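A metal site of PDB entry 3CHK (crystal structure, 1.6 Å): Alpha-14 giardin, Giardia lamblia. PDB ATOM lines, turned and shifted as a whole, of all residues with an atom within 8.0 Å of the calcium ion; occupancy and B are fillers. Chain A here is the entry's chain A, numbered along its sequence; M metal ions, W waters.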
ATOM      1  N   ALA A 219     -17.723 -31.806   9.263  1.00  0.00           N
ATOM      2  CA  ALA A 219     -18.768 -32.422   8.435  1.00  0.00           C
ATOM      3  C   ALA A 219     -20.173 -31.878   8.749  1.00  0.00           C
ATOM      4  O   ALA A 219     -20.987 -31.722   7.843  1.00  0.00           O
ATOM      5  CB  ALA A 219     -18.717 -33.966   8.537  1.00  0.00           C
ATOM      6  N   GLY A 220     -20.449 -31.569  10.019  1.00  0.00           N
ATOM      7  CA  GLY A 220     -21.708 -30.984  10.442  1.00  0.00           C
ATOM      8  C   GLY A 220     -21.874 -29.628   9.803  1.00  0.00           C
ATOM      9  O   GLY A 220     -22.951 -29.306   9.285  1.00  0.00           O
ATOM     10  N   VAL A 221     -20.789 -28.853   9.795  1.00  0.00           N
ATOM     11  CA  VAL A 221     -20.814 -27.516   9.135  1.00  0.00           C
ATOM     12  C   VAL A 221     -21.108 -27.655   7.642  1.00  0.00           C
ATOM     13  O   VAL A 221     -21.952 -26.925   7.089  1.00  0.00           O
ATOM     14  CB  VAL A 221     -19.440 -26.794   9.365  1.00  0.00           C
ATOM     15  CG1 VAL A 221     -19.342 -25.599   8.461  1.00  0.00           C
ATOM     16  CG2 VAL A 221     -19.277 -26.380  10.849  1.00  0.00           C
ATOM     17  N   GLU A 222     -20.435 -28.596   6.995  1.00  0.00           N
ATOM     18  CA  GLU A 222     -20.682 -28.892   5.589  1.00  0.00           C
ATOM     19  C   GLU A 222     -22.166 -29.213   5.310  1.00  0.00           C
ATOM     20  O   GLU A 222     -22.779 -28.662   4.367  1.00  0.00           O
ATOM     21  CB  GLU A 222     -19.779 -30.022   5.127  1.00  0.00           C
ATOM     22  CG  GLU A 222     -18.303 -29.662   5.048  1.00  0.00           C
ATOM     23  CD  GLU A 222     -17.479 -30.684   4.269  1.00  0.00           C
ATOM     24  OE1 GLU A 222     -17.603 -30.711   3.018  1.00  0.00           O
ATOM     25  OE2 GLU A 222     -16.693 -31.435   4.888  1.00  0.00           O
ATOM     26  N   ASP A 223     -22.735 -30.105   6.114  1.00  0.00           N
ATOM     27  CA  ASP A 223     -24.158 -30.490   6.048  1.00  0.00           C
ATOM     28  C   ASP A 223     -25.098 -29.283   6.197  1.00  0.00           C
ATOM     29  O   ASP A 223     -26.072 -29.152   5.438  1.00  0.00           O
ATOM     30  CB  ASP A 223     -24.521 -31.481   7.184  1.00  0.00           C
ATOM     31  CG  ASP A 223     -23.920 -32.869   7.023  1.00  0.00           C
ATOM     32  OD1 ASP A 223     -23.351 -33.168   5.959  1.00  0.00           O
ATOM     33  OD2 ASP A 223     -24.052 -33.676   8.018  1.00  0.00           O
ATOM     34  N   GLU A 224     -24.813 -28.418   7.177  1.00  0.00           N
ATOM     35  CA  GLU A 224     -25.744 -27.402   7.631  1.00  0.00           C
ATOM     36  C   GLU A 224     -25.789 -26.200   6.686  1.00  0.00           C
ATOM     37  O   GLU A 224     -26.872 -25.669   6.403  1.00  0.00           O
ATOM     38  CB  GLU A 224     -25.402 -26.970   9.079  1.00  0.00           C
ATOM     39  CG  GLU A 224     -26.332 -25.925   9.720  1.00  0.00           C
ATOM     40  CD  GLU A 224     -27.657 -26.502  10.262  1.00  0.00           C
ATOM     41  OE1 GLU A 224     -28.196 -27.434   9.623  1.00  0.00           O
ATOM     42  OE2 GLU A 224     -28.157 -26.021  11.274  1.00  0.00           O
ATOM     43  N   PHE A 225     -24.622 -25.793   6.196  1.00  0.00           N
ATOM     44  CA  PHE A 225     -24.491 -24.509   5.508  1.00  0.00           C
ATOM     45  C   PHE A 225     -24.182 -24.688   4.046  1.00  0.00           C
ATOM     46  O   PHE A 225     -23.700 -25.731   3.624  1.00  0.00           O
ATOM     47  CB  PHE A 225     -23.371 -23.687   6.177  1.00  0.00           C
ATOM     48  CG  PHE A 225     -23.637 -23.352   7.624  1.00  0.00           C
ATOM     49  CD1 PHE A 225     -24.523 -22.360   7.962  1.00  0.00           C
ATOM     50  CD2 PHE A 225     -22.965 -24.043   8.656  1.00  0.00           C
ATOM     51  CE1 PHE A 225     -24.789 -22.044   9.295  1.00  0.00           C
ATOM     52  CE2 PHE A 225     -23.234 -23.749   9.985  1.00  0.00           C
ATOM     53  CZ  PHE A 225     -24.136 -22.746  10.325  1.00  0.00           C
ATOM     54  N   GLN A 226     -24.471 -23.638   3.257  1.00  0.00           N
ATOM     55  CA  GLN A 226     -24.030 -23.615   1.878  1.00  0.00           C
ATOM     56  C   GLN A 226     -23.455 -22.239   1.534  1.00  0.00           C
ATOM     57  O   GLN A 226     -23.713 -21.262   2.242  1.00  0.00           O
ATOM     58  CB  GLN A 226     -25.188 -23.914   0.937  1.00  0.00           C
ATOM     59  CG  GLN A 226     -24.729 -24.795  -0.229  1.00  0.00           C
ATOM     60  CD  GLN A 226     -24.475 -26.228   0.216  1.00  0.00           C
ATOM     61  OE1 GLN A 226     -25.373 -26.886   0.741  1.00  0.00           O
ATOM     62  NE2 GLN A 226     -23.243 -26.722   0.021  1.00  0.00           N
ATOM     63  N   GLY A 227     -22.654 -22.206   0.455  1.00  0.00           N
ATOM     64  CA  GLY A 227     -22.123 -20.939  -0.089  1.00  0.00           C
ATOM     65  C   GLY A 227     -21.209 -20.233   0.883  1.00  0.00           C
ATOM     66  O   GLY A 227     -20.402 -20.872   1.560  1.00  0.00           O
ATOM     67  N   ASP A 229     -21.834 -18.887   3.771  1.00  0.00           N
ATOM     68  CA  ASP A 229     -22.051 -19.402   5.125  1.00  0.00           C
ATOM     69  C   ASP A 229     -21.103 -20.582   5.375  1.00  0.00           C
ATOM     70  O   ASP A 229     -20.437 -20.633   6.406  1.00  0.00           O
ATOM     71  CB  ASP A 229     -23.505 -19.908   5.333  1.00  0.00           C
ATOM     72  CG  ASP A 229     -24.543 -18.792   5.467  1.00  0.00           C
ATOM     73  OD1 ASP A 229     -24.197 -17.571   5.602  1.00  0.00           O
ATOM     74  OD2 ASP A 229     -25.761 -19.167   5.455  1.00  0.00           O
ATOM     75  N   GLU A 230     -21.071 -21.539   4.445  1.00  0.00           N
ATOM     76  CA  GLU A 230     -20.258 -22.748   4.617  1.00  0.00           C
ATOM     77  C   GLU A 230     -18.769 -22.407   4.677  1.00  0.00           C
ATOM     78  O   GLU A 230     -18.044 -22.889   5.551  1.00  0.00           O
ATOM     79  CB  GLU A 230     -20.552 -23.772   3.522  1.00  0.00           C
ATOM     80  CG  GLU A 230     -19.796 -25.072   3.740  1.00  0.00           C
ATOM     81  CD  GLU A 230     -20.021 -26.083   2.647  1.00  0.00           C
ATOM     82  OE1 GLU A 230     -21.186 -26.228   2.206  1.00  0.00           O
ATOM     83  OE2 GLU A 230     -19.035 -26.716   2.244  1.00  0.00           O
ATOM     84  N   TYR A 231     -18.313 -21.542   3.766  1.00  0.00           N
ATOM     85  CA  TYR A 231     -16.928 -21.103   3.810  1.00  0.00           C
ATOM     86  C   TYR A 231     -16.592 -20.429   5.155  1.00  0.00           C
ATOM     87  O   TYR A 231     -15.533 -20.720   5.779  1.00  0.00           O
ATOM     88  CB  TYR A 231     -16.638 -20.140   2.628  1.00  0.00           C
ATOM     89  CG  TYR A 231     -15.233 -19.588   2.720  1.00  0.00           C
ATOM     90  CD1 TYR A 231     -14.144 -20.328   2.241  1.00  0.00           C
ATOM     91  CD2 TYR A 231     -14.999 -18.329   3.306  1.00  0.00           C
ATOM     92  CE1 TYR A 231     -12.818 -19.821   2.336  1.00  0.00           C
ATOM     93  CE2 TYR A 231     -13.684 -17.803   3.413  1.00  0.00           C
ATOM     94  CZ  TYR A 231     -12.587 -18.549   2.933  1.00  0.00           C
ATOM     95  OH  TYR A 231     -11.280 -18.083   2.991  1.00  0.00           O
ATOM     96  N   LYS A 234     -16.575 -23.048   8.053  1.00  0.00           N
ATOM     97  CA  LYS A 234     -15.379 -23.894   7.923  1.00  0.00           C
ATOM     98  C   LYS A 234     -14.125 -23.100   8.284  1.00  0.00           C
ATOM     99  O   LYS A 234     -13.223 -23.658   8.885  1.00  0.00           O
ATOM    100  CB  LYS A 234     -15.240 -24.520   6.540  1.00  0.00           C
ATOM    101  CG  LYS A 234     -16.291 -25.560   6.233  1.00  0.00           C
ATOM    102  CD  LYS A 234     -16.161 -25.972   4.782  1.00  0.00           C
ATOM    103  CE  LYS A 234     -16.738 -27.325   4.553  1.00  0.00           C
ATOM    104  NZ  LYS A 234     -16.826 -27.720   3.093  1.00  0.00           N
HETATM  105 CA    CA M   1     -23.100 -27.628   2.329  1.00  0.00          CA
HETATM  106  O   HOH W   1     -24.076 -30.213   1.881  1.00  0.00           O
HETATM  107  O   HOH W   2     -22.069 -28.944   1.354  1.00  0.00           O
HETATM  108  O   HOH W   3     -25.620 -27.950   2.727  1.00  0.00           O
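The calcium ion is bound by water W2 (1.9 Å), O of Glu 222 (2.3 Å), O of Phe 225 (2.4 Å), OE1 of Glu 230 (2.4 Å), NE2 of Gln 226 (2.5 Å), water W3 (2.6 Å), water W1 (2.8 Å) and OE1 of Gln 226 (2.9 Å).
The calcium ion has eight donor atoms within binding distance.
The side-chain carboxylate (OE1) of Glu 222 is in salt-bridge range of the side-chain amino group (NZ) of Lys 234 (3.1 Å).
The side-chain amino group (NZ) of Lys 234 is in salt-bridge range of the side-chain carboxylate (OE2) of Glu 230 (2.6 Å).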
